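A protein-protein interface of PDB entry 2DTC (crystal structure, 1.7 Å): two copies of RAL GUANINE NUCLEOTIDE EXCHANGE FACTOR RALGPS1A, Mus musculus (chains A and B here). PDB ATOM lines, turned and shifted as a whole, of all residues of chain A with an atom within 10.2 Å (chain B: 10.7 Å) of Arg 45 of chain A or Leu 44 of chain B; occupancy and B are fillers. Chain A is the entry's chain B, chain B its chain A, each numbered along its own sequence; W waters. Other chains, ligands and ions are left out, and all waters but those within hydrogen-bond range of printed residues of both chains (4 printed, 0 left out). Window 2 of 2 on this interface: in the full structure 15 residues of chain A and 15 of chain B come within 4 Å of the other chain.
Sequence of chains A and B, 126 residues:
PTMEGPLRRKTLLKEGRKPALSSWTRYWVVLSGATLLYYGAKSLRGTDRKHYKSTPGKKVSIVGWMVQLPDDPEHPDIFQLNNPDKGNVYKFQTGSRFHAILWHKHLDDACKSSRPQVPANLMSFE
The side-chain hydroxyl (OG) of Ser 43 of chain B is in hydrogen-bond range of the backbone NH (N) of Arg 45 of chain B (3.4 Å).
The backbone carbonyl oxygen (O) of Arg 45 of chain B lies close to a ring nitrogen (ND1) of His 51 of chain B, 3.4 Å away.
The backbone carbonyl oxygen (O) of Arg 45 of chain A lies within hydrogen-bond range of the side-chain hydroxyl (OG) of Ser 43 of chain A, 2.9 Å away.
A ring nitrogen (ND1) of His 51 of chain A is in hydrogen-bond range of the backbone NH (N) of Thr 47 of chain A (3.1 Å).
The backbone NH of Asp 48 of chain A sits at hydrogen-bond distance from a ring nitrogen (ND1) of His 51 of chain A (3.0 Å).
Water W4 lies within hydrogen-bond range of OD1 of Asp 48 of chain A (2.7 Å) and NH1 of Arg 8 of chain B (3.5 Å).
Water W1 bridges the side-chain carboxylate (OD2) of Asp 48 of chain B (2.7 Å) and the guanidinium group (NH2) of Arg 8 of chain A (3.4 Å).
Water W2 bridges the backbone NH (N) of Gly 46 of chain B (2.9 Å) and the guanidinium group (NH2) of Arg 45 of chain A (3.1 Å).
Water W3 lies within hydrogen-bond range of O of Gly 46 of chain B, OG1 of Thr 47 of chain B and OG1 of Thr 47 of chain A.
Arg 45 of chain B touches Arg 45 of chain A (CA to NH2, 3.4 Å).
Of the 17 printed residues of chain B, 5 touch a printed residue of chain A.
Among the printed residues, 5 pairs touch across the chains.
Among the printed residues, Asp or Glu carboxylates within 4 Å of a Lys or Arg side-chain nitrogen of the other chain: Arg 8 of chain A with Asp 48 of chain B (2.8 Å) and Asp 48 of chain A with Arg 8 of chain B (2.7 Å).
Arg 8 of chain A touches Asp 48 of chain B, and with the chains exchanged Asp 48 of chain A touches Arg 8 of chain B.
Arg 45 of chain A touches Leu 44 of chain B, but with the chains exchanged Leu 44 of chain A does not touch Arg 45 of chain B (7.4 Å).
Arg 45 of chain B touches its own counterpart, Arg 45 of chain A.
Thr 47 of chain B touches its own counterpart, Thr 47 of chain A.
The guanidinium group of Arg 8 of chain B is in salt-bridge range of the side-chain carboxylate of Asp 48 of chain A (2.7 Å).
The guanidinium group (NH2) of Arg 45 of chain A is in hydrogen-bond range of the backbone carbonyl oxygen (O) of Leu 44 of chain B, at 3.3 Å.
The side-chain hydroxyl (OG1) of Thr 47 of chain A lies within hydrogen-bond range of the side-chain hydroxyl (OG1) of Thr 47 of chain B (2.7 Å).
OD2 of Asp 48 of chain B lies within salt-bridge range of NH2 of Arg 8 of chain A, 2.8 Å away.
Of the printed residues of chain B, Arg 8 of chain A touches Asp 48.
No residue of chain B comes within 4 Å of Ser 43 of chain A.
Of the printed residues of chain B, Arg 45 of chain A touches Leu 44 (3.3 Å) and Arg 45 (3.4 Å).
No residue of chain B comes within 4 Å of Gly 46 of chain A.
Printed residues of chain B within 4 Å of Asp 48 of chain A: Arg 8.
No residue of chain B comes within 4 Å of His 51 of chain A.
Ala 41 of chain B touches none of the printed residues of chain A.
No residue of chain A comes within 4 Å of Ser 43 of chain B.
Of the printed residues of chain A, Arg 45 of chain B touches Arg 45 (3.4 Å).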
ATOM      1  N   PRO A   6      14.553  -0.152 -36.197  1.00  0.00           N
ATOM      2  CA  PRO A   6      14.769  -1.580 -36.305  1.00  0.00           C
ATOM      3  C   PRO A   6      13.452  -2.262 -36.642  1.00  0.00           C
ATOM      4  O   PRO A   6      12.456  -2.078 -35.944  1.00  0.00           O
ATOM      5  CB  PRO A   6      15.287  -1.957 -34.929  1.00  0.00           C
ATOM      6  CG  PRO A   6      14.573  -0.996 -34.021  1.00  0.00           C
ATOM      7  CD  PRO A   6      14.577   0.293 -34.786  1.00  0.00           C
ATOM      8  N   ARG A   8      11.616  -6.077 -38.305  1.00  0.00           N
ATOM      9  CA  ARG A   8      11.790  -7.451 -38.754  1.00  0.00           C
ATOM     10  C   ARG A   8      10.834  -7.577 -39.930  1.00  0.00           C
ATOM     11  O   ARG A   8       9.691  -7.132 -39.848  1.00  0.00           O
ATOM     12  CB  ARG A   8      11.406  -8.464 -37.663  1.00  0.00           C
ATOM     13  CG  ARG A   8      12.454  -8.626 -36.588  1.00  0.00           C
ATOM     14  CD  ARG A   8      12.175  -7.743 -35.376  1.00  0.00           C
ATOM     15  NE  ARG A   8      11.038  -8.215 -34.583  1.00  0.00           N
ATOM     16  CZ  ARG A   8      10.709  -7.710 -33.394  1.00  0.00           C
ATOM     17  NH1 ARG A   8      11.435  -6.729 -32.876  1.00  0.00           N
ATOM     18  NH2 ARG A   8       9.654  -8.171 -32.725  1.00  0.00           N
ATOM     19  N   ARG A  26      15.858  -9.737 -39.306  1.00  0.00           N
ATOM     20  CA  ARG A  26      16.135  -8.459 -38.634  1.00  0.00           C
ATOM     21  C   ARG A  26      16.888  -7.455 -39.531  1.00  0.00           C
ATOM     22  O   ARG A  26      17.906  -7.786 -40.155  1.00  0.00           O
ATOM     23  CB  ARG A  26      16.948  -8.707 -37.359  1.00  0.00           C
ATOM     24  CG  ARG A  26      16.200  -9.495 -36.302  1.00  0.00           C
ATOM     25  CD  ARG A  26      17.145 -10.063 -35.254  1.00  0.00           C
ATOM     26  NE  ARG A  26      17.982  -9.016 -34.677  1.00  0.00           N
ATOM     27  CZ  ARG A  26      19.309  -9.012 -34.747  1.00  0.00           C
ATOM     28  NH1 ARG A  26      19.945 -10.000 -35.362  1.00  0.00           N
ATOM     29  NH2 ARG A  26      19.999  -8.021 -34.203  1.00  0.00           N
ATOM     30  N   TYR A  27      16.415  -6.209 -39.551  1.00  0.00           N
ATOM     31  CA  TYR A  27      17.035  -5.157 -40.365  1.00  0.00           C
ATOM     32  C   TYR A  27      16.933  -3.810 -39.682  1.00  0.00           C
ATOM     33  O   TYR A  27      16.105  -3.620 -38.784  1.00  0.00           O
ATOM     34  CB  TYR A  27      16.292  -4.947 -41.702  1.00  0.00           C
ATOM     35  CG  TYR A  27      16.336  -6.055 -42.719  1.00  0.00           C
ATOM     36  CD1 TYR A  27      17.469  -6.282 -43.473  1.00  0.00           C
ATOM     37  CD2 TYR A  27      15.232  -6.876 -42.916  1.00  0.00           C
ATOM     38  CE1 TYR A  27      17.514  -7.320 -44.415  1.00  0.00           C
ATOM     39  CE2 TYR A  27      15.258  -7.917 -43.850  1.00  0.00           C
ATOM     40  CZ  TYR A  27      16.398  -8.130 -44.590  1.00  0.00           C
ATOM     41  OH  TYR A  27      16.405  -9.156 -45.505  1.00  0.00           O
ATOM     42  N   GLY A  40      21.388  -5.132 -43.062  1.00  0.00           N
ATOM     43  CA  GLY A  40      21.307  -6.382 -42.331  1.00  0.00           C
ATOM     44  C   GLY A  40      21.950  -6.360 -40.949  1.00  0.00           C
ATOM     45  O   GLY A  40      22.747  -5.481 -40.633  1.00  0.00           O
ATOM     46  N   ALA A  41      21.599  -7.333 -40.119  1.00  0.00           N
ATOM     47  CA  ALA A  41      22.163  -7.408 -38.770  1.00  0.00           C
ATOM     48  C   ALA A  41      23.639  -7.833 -38.742  1.00  0.00           C
ATOM     49  O   ALA A  41      24.098  -8.570 -39.612  1.00  0.00           O
ATOM     50  CB  ALA A  41      21.332  -8.364 -37.923  1.00  0.00           C
ATOM     51  N   LYS A  42      24.374  -7.351 -37.747  1.00  0.00           N
ATOM     52  CA  LYS A  42      25.791  -7.708 -37.582  1.00  0.00           C
ATOM     53  C   LYS A  42      25.898  -8.922 -36.668  1.00  0.00           C
ATOM     54  O   LYS A  42      26.846  -9.707 -36.778  1.00  0.00           O
ATOM     55  CB  LYS A  42      26.581  -6.576 -36.929  1.00  0.00           C
ATOM     56  CG  LYS A  42      26.876  -5.372 -37.773  1.00  0.00           C
ATOM     57  CD  LYS A  42      27.700  -4.389 -36.937  1.00  0.00           C
ATOM     58  CE  LYS A  42      28.077  -3.138 -37.699  1.00  0.00           C
ATOM     59  NZ  LYS A  42      28.658  -2.113 -36.778  1.00  0.00           N
ATOM     60  N   SER A  43      24.936  -9.056 -35.756  1.00  0.00           N
ATOM     61  CA  SER A  43      24.903 -10.165 -34.802  1.00  0.00           C
ATOM     62  C   SER A  43      23.500 -10.764 -34.738  1.00  0.00           C
ATOM     63  O   SER A  43      22.658 -10.460 -35.576  1.00  0.00           O
ATOM     64  CB  SER A  43      25.323  -9.683 -33.408  1.00  0.00           C
ATOM     65  OG  SER A  43      24.437  -8.694 -32.897  1.00  0.00           O
ATOM     66  N   LEU A  44      23.249 -11.603 -33.737  1.00  0.00           N
ATOM     67  CA  LEU A  44      21.944 -12.247 -33.590  1.00  0.00           C
ATOM     68  C   LEU A  44      21.008 -11.501 -32.650  1.00  0.00           C
ATOM     69  O   LEU A  44      19.836 -11.861 -32.527  1.00  0.00           O
ATOM     70  CB  LEU A  44      22.113 -13.674 -33.059  1.00  0.00           C
ATOM     71  CG  LEU A  44      22.808 -14.715 -33.932  1.00  0.00           C
ATOM     72  CD1 LEU A  44      23.044 -15.969 -33.107  1.00  0.00           C
ATOM     73  CD2 LEU A  44      21.952 -15.027 -35.157  1.00  0.00           C
ATOM     74  N   ARG A  45      21.519 -10.472 -31.982  1.00  0.00           N
ATOM     75  CA  ARG A  45      20.704  -9.729 -31.022  1.00  0.00           C
ATOM     76  C   ARG A  45      21.066  -8.244 -31.028  1.00  0.00           C
ATOM     77  O   ARG A  45      22.219  -7.874 -31.291  1.00  0.00           O
ATOM     78  CB  ARG A  45      20.917 -10.311 -29.610  1.00  0.00           C
ATOM     79  CG  ARG A  45      20.025  -9.715 -28.511  1.00  0.00           C
ATOM     80  CD  ARG A  45      20.291 -10.354 -27.132  1.00  0.00           C
ATOM     81  NE  ARG A  45      19.337  -9.897 -26.118  1.00  0.00           N
ATOM     82  CZ  ARG A  45      19.323 -10.310 -24.851  1.00  0.00           C
ATOM     83  NH1 ARG A  45      20.218 -11.193 -24.431  1.00  0.00           N
ATOM     84  NH2 ARG A  45      18.406  -9.848 -24.002  1.00  0.00           N
ATOM     85  N   GLY A  46      20.081  -7.395 -30.757  1.00  0.00           N
ATOM     86  CA  GLY A  46      20.349  -5.967 -30.718  1.00  0.00           C
ATOM     87  C   GLY A  46      19.468  -5.175 -31.658  1.00  0.00           C
ATOM     88  O   GLY A  46      19.220  -5.612 -32.787  1.00  0.00           O
ATOM     89  N   THR A  47      18.983  -4.022 -31.193  1.00  0.00           N
ATOM     90  CA  THR A  47      18.131  -3.170 -32.021  1.00  0.00           C
ATOM     91  C   THR A  47      18.644  -1.732 -32.158  1.00  0.00           C
ATOM     92  O   THR A  47      17.912  -0.877 -32.652  1.00  0.00           O
ATOM     93  CB  THR A  47      16.693  -3.087 -31.481  1.00  0.00           C
ATOM     94  OG1 THR A  47      16.743  -2.795 -30.078  1.00  0.00           O
ATOM     95  CG2 THR A  47      15.935  -4.408 -31.745  1.00  0.00           C
ATOM     96  N   ASP A  48      19.869  -1.460 -31.719  1.00  0.00           N
ATOM     97  CA  ASP A  48      20.451  -0.119 -31.855  1.00  0.00           C
ATOM     98  C   ASP A  48      21.018  -0.036 -33.289  1.00  0.00           C
ATOM     99  O   ASP A  48      21.315  -1.071 -33.914  1.00  0.00           O
ATOM    100  CB  ASP A  48      21.624   0.098 -30.891  1.00  0.00           C
ATOM    101  CG  ASP A  48      21.201   0.312 -29.435  1.00  0.00           C
ATOM    102  OD1 ASP A  48      20.006   0.140 -29.081  1.00  0.00           O
ATOM    103  OD2 ASP A  48      22.111   0.652 -28.641  1.00  0.00           O
ATOM    104  N   ARG A  49      21.200   1.178 -33.797  1.00  0.00           N
ATOM    105  CA  ARG A  49      21.728   1.333 -35.148  1.00  0.00           C
ATOM    106  C   ARG A  49      23.063   0.579 -35.324  1.00  0.00           C
ATOM    107  O   ARG A  49      23.300  -0.049 -36.366  1.00  0.00           O
ATOM    108  CB  ARG A  49      21.929   2.814 -35.479  1.00  0.00           C
ATOM    109  CG  ARG A  49      22.547   3.064 -36.873  1.00  0.00           C
ATOM    110  CD  ARG A  49      21.638   2.542 -37.963  1.00  0.00           C
ATOM    111  NE  ARG A  49      22.196   2.671 -39.306  1.00  0.00           N
ATOM    112  CZ  ARG A  49      22.935   1.757 -39.934  1.00  0.00           C
ATOM    113  NH1 ARG A  49      23.260   0.600 -39.351  1.00  0.00           N
ATOM    114  NH2 ARG A  49      23.294   1.977 -41.194  1.00  0.00           N
ATOM    115  N   LYS A  50      23.901   0.612 -34.296  1.00  0.00           N
ATOM    116  CA  LYS A  50      25.212  -0.039 -34.324  1.00  0.00           C
ATOM    117  C   LYS A  50      25.168  -1.567 -34.457  1.00  0.00           C
ATOM    118  O   LYS A  50      26.180  -2.183 -34.784  1.00  0.00           O
ATOM    119  CB  LYS A  50      26.017   0.356 -33.070  1.00  0.00           C
ATOM    120  CG  LYS A  50      25.430  -0.179 -31.760  1.00  0.00           C
ATOM    121  CD  LYS A  50      26.178   0.387 -30.546  1.00  0.00           C
ATOM    122  CE  LYS A  50      25.793  -0.335 -29.265  1.00  0.00           C
ATOM    123  NZ  LYS A  50      26.264  -1.749 -29.254  1.00  0.00           N
ATOM    124  N   HIS A  51      24.009  -2.177 -34.211  1.00  0.00           N
ATOM    125  CA  HIS A  51      23.885  -3.624 -34.347  1.00  0.00           C
ATOM    126  C   HIS A  51      23.627  -4.023 -35.802  1.00  0.00           C
ATOM    127  O   HIS A  51      23.437  -5.206 -36.090  1.00  0.00           O
ATOM    128  CB  HIS A  51      22.756  -4.148 -33.447  1.00  0.00           C
ATOM    129  CG  HIS A  51      23.010  -3.935 -31.984  1.00  0.00           C
ATOM    130  ND1 HIS A  51      22.070  -3.401 -31.128  1.00  0.00           N
ATOM    131  CD2 HIS A  51      24.112  -4.168 -31.232  1.00  0.00           C
ATOM    132  CE1 HIS A  51      22.582  -3.310 -29.913  1.00  0.00           C
ATOM    133  NE2 HIS A  51      23.821  -3.770 -29.948  1.00  0.00           N
ATOM    134  N   TYR A  52      23.611  -3.046 -36.713  1.00  0.00           N
ATOM    135  CA  TYR A  52      23.358  -3.325 -38.123  1.00  0.00           C
ATOM    136  C   TYR A  52      24.465  -2.781 -39.026  1.00  0.00           C
ATOM    137  O   TYR A  52      25.184  -1.858 -38.654  1.00  0.00           O
ATOM    138  CB  TYR A  52      21.982  -2.752 -38.509  1.00  0.00           C
ATOM    139  CG  TYR A  52      20.856  -3.382 -37.710  1.00  0.00           C
ATOM    140  CD1 TYR A  52      20.243  -4.564 -38.135  1.00  0.00           C
ATOM    141  CD2 TYR A  52      20.447  -2.839 -36.485  1.00  0.00           C
ATOM    142  CE1 TYR A  52      19.251  -5.185 -37.359  1.00  0.00           C
ATOM    143  CE2 TYR A  52      19.484  -3.457 -35.713  1.00  0.00           C
ATOM    144  CZ  TYR A  52      18.892  -4.623 -36.152  1.00  0.00           C
ATOM    145  OH  TYR A  52      17.944  -5.242 -35.363  1.00  0.00           O
ATOM    146  N   ARG B   8      17.254   4.183 -22.559  1.00  0.00           N
ATOM    147  CA  ARG B   8      18.082   3.862 -21.398  1.00  0.00           C
ATOM    148  C   ARG B   8      18.323   5.224 -20.771  1.00  0.00           C
ATOM    149  O   ARG B   8      18.651   6.184 -21.476  1.00  0.00           O
ATOM    150  CB  ARG B   8      19.433   3.253 -21.780  1.00  0.00           C
ATOM    151  CG  ARG B   8      19.388   1.748 -22.004  1.00  0.00           C
ATOM    152  CD  ARG B   8      19.235   1.383 -23.484  1.00  0.00           C
ATOM    153  NE  ARG B   8      20.389   1.789 -24.295  1.00  0.00           N
ATOM    154  CZ  ARG B   8      20.561   1.434 -25.568  1.00  0.00           C
ATOM    155  NH1 ARG B   8      19.658   0.668 -26.169  1.00  0.00           N
ATOM    156  NH2 ARG B   8      21.624   1.846 -26.240  1.00  0.00           N
ATOM    157  N   THR B  25      19.793   2.513 -17.095  1.00  0.00           N
ATOM    158  CA  THR B  25      18.664   1.640 -16.753  1.00  0.00           C
ATOM    159  C   THR B  25      17.716   1.611 -17.934  1.00  0.00           C
ATOM    160  O   THR B  25      17.400   2.661 -18.476  1.00  0.00           O
ATOM    161  CB  THR B  25      17.903   2.168 -15.540  1.00  0.00           C
ATOM    162  OG1 THR B  25      18.806   2.240 -14.437  1.00  0.00           O
ATOM    163  CG2 THR B  25      16.713   1.243 -15.175  1.00  0.00           C
ATOM    164  N   ARG B  26      17.260   0.414 -18.311  1.00  0.00           N
ATOM    165  CA  ARG B  26      16.348   0.234 -19.447  1.00  0.00           C
ATOM    166  C   ARG B  26      14.878   0.484 -19.088  1.00  0.00           C
ATOM    167  O   ARG B  26      14.366  -0.054 -18.094  1.00  0.00           O
ATOM    168  CB  ARG B  26      16.498  -1.183 -20.006  1.00  0.00           C
ATOM    169  CG  ARG B  26      17.859  -1.482 -20.617  1.00  0.00           C
ATOM    170  CD  ARG B  26      17.914  -2.960 -21.024  1.00  0.00           C
ATOM    171  NE  ARG B  26      17.641  -3.819 -19.878  1.00  0.00           N
ATOM    172  CZ  ARG B  26      16.675  -4.738 -19.838  1.00  0.00           C
ATOM    173  NH1 ARG B  26      15.881  -4.926 -20.888  1.00  0.00           N
ATOM    174  NH2 ARG B  26      16.507  -5.467 -18.744  1.00  0.00           N
ATOM    175  N   TYR B  27      14.192   1.263 -19.926  1.00  0.00           N
ATOM    176  CA  TYR B  27      12.791   1.589 -19.721  1.00  0.00           C
ATOM    177  C   TYR B  27      12.025   1.671 -21.024  1.00  0.00           C
ATOM    178  O   TYR B  27      12.617   1.894 -22.098  1.00  0.00           O
ATOM    179  CB  TYR B  27      12.616   2.992 -19.101  1.00  0.00           C
ATOM    180  CG  TYR B  27      13.087   3.186 -17.689  1.00  0.00           C
ATOM    181  CD1 TYR B  27      12.390   2.644 -16.619  1.00  0.00           C
ATOM    182  CD2 TYR B  27      14.241   3.910 -17.428  1.00  0.00           C
ATOM    183  CE1 TYR B  27      12.837   2.819 -15.301  1.00  0.00           C
ATOM    184  CE2 TYR B  27      14.704   4.087 -16.119  1.00  0.00           C
ATOM    185  CZ  TYR B  27      13.994   3.539 -15.068  1.00  0.00           C
ATOM    186  OH  TYR B  27      14.459   3.715 -13.793  1.00  0.00           O
ATOM    187  N   GLY B  40       9.481  -0.190 -16.272  1.00  0.00           N
ATOM    188  CA  GLY B  40      10.733  -0.911 -16.177  1.00  0.00           C
ATOM    189  C   GLY B  40      10.757  -2.203 -16.969  1.00  0.00           C
ATOM    190  O   GLY B  40       9.704  -2.708 -17.400  1.00  0.00           O
ATOM    191  N   ALA B  41      11.944  -2.771 -17.152  1.00  0.00           N
ATOM    192  CA  ALA B  41      12.039  -4.025 -17.906  1.00  0.00           C
ATOM    193  C   ALA B  41      11.505  -5.203 -17.089  1.00  0.00           C
ATOM    194  O   ALA B  41      11.683  -5.255 -15.861  1.00  0.00           O
ATOM    195  CB  ALA B  41      13.486  -4.296 -18.320  1.00  0.00           C
ATOM    196  N   LYS B  42      10.847  -6.141 -17.763  1.00  0.00           N
ATOM    197  CA  LYS B  42      10.303  -7.321 -17.066  1.00  0.00           C
ATOM    198  C   LYS B  42      11.461  -8.247 -16.749  1.00  0.00           C
ATOM    199  O   LYS B  42      11.527  -8.863 -15.674  1.00  0.00           O
ATOM    200  CB  LYS B  42       9.320  -8.082 -17.947  1.00  0.00           C
ATOM    201  CG  LYS B  42       7.928  -7.530 -18.007  1.00  0.00           C
ATOM    202  CD  LYS B  42       7.119  -8.345 -18.995  1.00  0.00           C
ATOM    203  CE  LYS B  42       5.736  -7.759 -19.201  1.00  0.00           C
ATOM    204  NZ  LYS B  42       5.025  -8.482 -20.291  1.00  0.00           N
ATOM    205  N   SER B  43      12.388  -8.339 -17.688  1.00  0.00           N
ATOM    206  CA  SER B  43      13.534  -9.207 -17.493  1.00  0.00           C
ATOM    207  C   SER B  43      14.800  -8.659 -18.131  1.00  0.00           C
ATOM    208  O   SER B  43      15.056  -7.457 -18.139  1.00  0.00           O
ATOM    209  CB  SER B  43      13.234 -10.594 -18.064  1.00  0.00           C
ATOM    210  OG  SER B  43      13.032 -10.519 -19.467  1.00  0.00           O
ATOM    211  N   LEU B  44      15.591  -9.560 -18.679  1.00  0.00           N
ATOM    212  CA  LEU B  44      16.848  -9.181 -19.293  1.00  0.00           C
ATOM    213  C   LEU B  44      16.658  -8.856 -20.777  1.00  0.00           C
ATOM    214  O   LEU B  44      17.435  -8.113 -21.359  1.00  0.00           O
ATOM    215  CB  LEU B  44      17.829 -10.337 -19.159  1.00  0.00           C
ATOM    216  CG  LEU B  44      18.204 -10.806 -17.752  1.00  0.00           C
ATOM    217  CD1 LEU B  44      19.238 -11.929 -17.898  1.00  0.00           C
ATOM    218  CD2 LEU B  44      18.807  -9.642 -16.957  1.00  0.00           C
ATOM    219  N   ARG B  45      15.617  -9.432 -21.366  1.00  0.00           N
ATOM    220  CA  ARG B  45      15.312  -9.273 -22.792  1.00  0.00           C
ATOM    221  C   ARG B  45      14.451  -8.040 -22.985  1.00  0.00           C
ATOM    222  O   ARG B  45      13.247  -8.097 -22.731  1.00  0.00           O
ATOM    223  CB  ARG B  45      14.556 -10.522 -23.271  1.00  0.00           C
ATOM    224  CG  ARG B  45      14.160 -10.519 -24.728  1.00  0.00           C
ATOM    225  CD  ARG B  45      15.173 -11.242 -25.580  1.00  0.00           C
ATOM    226  NE  ARG B  45      14.792 -11.207 -26.987  1.00  0.00           N
ATOM    227  CZ  ARG B  45      13.671 -11.730 -27.476  1.00  0.00           C
ATOM    228  NH1 ARG B  45      12.809 -12.340 -26.673  1.00  0.00           N
ATOM    229  NH2 ARG B  45      13.406 -11.630 -28.773  1.00  0.00           N
ATOM    230  N   GLY B  46      15.027  -6.934 -23.456  1.00  0.00           N
ATOM    231  CA  GLY B  46      14.207  -5.742 -23.576  1.00  0.00           C
ATOM    232  C   GLY B  46      14.208  -4.790 -24.749  1.00  0.00           C
ATOM    233  O   GLY B  46      14.740  -3.692 -24.646  1.00  0.00           O
ATOM    234  N   THR B  47      13.604  -5.176 -25.869  1.00  0.00           N
ATOM    235  CA  THR B  47      13.533  -4.257 -26.989  1.00  0.00           C
ATOM    236  C   THR B  47      12.080  -3.889 -27.394  1.00  0.00           C
ATOM    237  O   THR B  47      11.791  -2.737 -27.722  1.00  0.00           O
ATOM    238  CB  THR B  47      14.317  -4.824 -28.197  1.00  0.00           C
ATOM    239  OG1 THR B  47      14.382  -3.815 -29.209  1.00  0.00           O
ATOM    240  CG2 THR B  47      13.670  -6.143 -28.741  1.00  0.00           C
ATOM    241  N   ASP B  48      11.168  -4.853 -27.328  1.00  0.00           N
ATOM    242  CA  ASP B  48       9.772  -4.649 -27.707  1.00  0.00           C
ATOM    243  C   ASP B  48       8.958  -4.167 -26.512  1.00  0.00           C
ATOM    244  O   ASP B  48       9.363  -4.357 -25.361  1.00  0.00           O
ATOM    245  CB  ASP B  48       9.169  -5.961 -28.202  1.00  0.00           C
ATOM    246  CG  ASP B  48       9.816  -6.468 -29.495  1.00  0.00           C
ATOM    247  OD1 ASP B  48      10.784  -5.842 -29.998  1.00  0.00           O
ATOM    248  OD2 ASP B  48       9.342  -7.511 -29.997  1.00  0.00           O
ATOM    249  N   LYS B  50       6.396  -5.403 -25.171  1.00  0.00           N
ATOM    250  CA  LYS B  50       6.038  -6.520 -24.297  1.00  0.00           C
ATOM    251  C   LYS B  50       7.166  -6.930 -23.362  1.00  0.00           C
ATOM    252  O   LYS B  50       6.945  -7.732 -22.455  1.00  0.00           O
ATOM    253  CB  LYS B  50       5.611  -7.736 -25.118  1.00  0.00           C
ATOM    254  CG  LYS B  50       6.729  -8.336 -25.930  1.00  0.00           C
ATOM    255  CD  LYS B  50       6.230  -9.483 -26.797  1.00  0.00           C
ATOM    256  CE  LYS B  50       7.359 -10.065 -27.643  1.00  0.00           C
ATOM    257  NZ  LYS B  50       6.840 -11.015 -28.668  1.00  0.00           N
ATOM    258  N   HIS B  51       8.364  -6.394 -23.582  1.00  0.00           N
ATOM    259  CA  HIS B  51       9.492  -6.731 -22.726  1.00  0.00           C
ATOM    260  C   HIS B  51       9.518  -5.853 -21.491  1.00  0.00           C
ATOM    261  O   HIS B  51      10.391  -6.027 -20.634  1.00  0.00           O
ATOM    262  CB  HIS B  51      10.830  -6.573 -23.470  1.00  0.00           C
ATOM    263  CG  HIS B  51      10.997  -7.500 -24.640  1.00  0.00           C
ATOM    264  ND1 HIS B  51      10.567  -8.810 -24.624  1.00  0.00           N
ATOM    265  CD2 HIS B  51      11.581  -7.312 -25.848  1.00  0.00           C
ATOM    266  CE1 HIS B  51      10.872  -9.386 -25.775  1.00  0.00           C
ATOM    267  NE2 HIS B  51      11.489  -8.498 -26.533  1.00  0.00           N
ATOM    268  N   TYR B  52       8.579  -4.909 -21.402  1.00  0.00           N
ATOM    269  CA  TYR B  52       8.509  -3.997 -20.272  1.00  0.00           C
ATOM    270  C   TYR B  52       7.177  -4.125 -19.549  1.00  0.00           C
ATOM    271  O   TYR B  52       6.165  -4.532 -20.127  1.00  0.00           O
ATOM    272  CB  TYR B  52       8.713  -2.552 -20.751  1.00  0.00           C
ATOM    273  CG  TYR B  52      10.075  -2.372 -21.376  1.00  0.00           C
ATOM    274  CD1 TYR B  52      11.166  -1.972 -20.605  1.00  0.00           C
ATOM    275  CD2 TYR B  52      10.291  -2.654 -22.727  1.00  0.00           C
ATOM    276  CE1 TYR B  52      12.442  -1.848 -21.166  1.00  0.00           C
ATOM    277  CE2 TYR B  52      11.555  -2.547 -23.289  1.00  0.00           C
ATOM    278  CZ  TYR B  52      12.623  -2.143 -22.503  1.00  0.00           C
ATOM    279  OH  TYR B  52      13.878  -2.046 -23.052  1.00  0.00           O
ATOM    280  N   LYS B  53       7.180  -3.737 -18.280  1.00  0.00           N
ATOM    281  CA  LYS B  53       6.010  -3.857 -17.439  1.00  0.00           C
ATOM    282  C   LYS B  53       4.775  -3.111 -17.903  1.00  0.00           C
ATOM    283  O   LYS B  53       4.856  -2.170 -18.691  1.00  0.00           O
ATOM    284  CB  LYS B  53       6.377  -3.463 -16.002  1.00  0.00           C
ATOM    285  CG  LYS B  53       7.319  -4.502 -15.395  1.00  0.00           C
ATOM    286  CD  LYS B  53       7.993  -4.038 -14.098  1.00  0.00           C
ATOM    287  CE  LYS B  53       9.018  -5.080 -13.676  1.00  0.00           C
ATOM    288  NZ  LYS B  53       9.724  -4.751 -12.398  1.00  0.00           N
HETATM  289  O   HOH W   1      10.022 -10.160 -29.960  1.00  0.00           O
HETATM  290  O   HOH W   2      16.824  -7.719 -25.563  1.00  0.00           O
HETATM  291  O   HOH W   3      15.958  -1.965 -26.813  1.00  0.00           O
HETATM  292  O   HOH W   4      17.468   1.030 -28.846  1.00  0.00           O
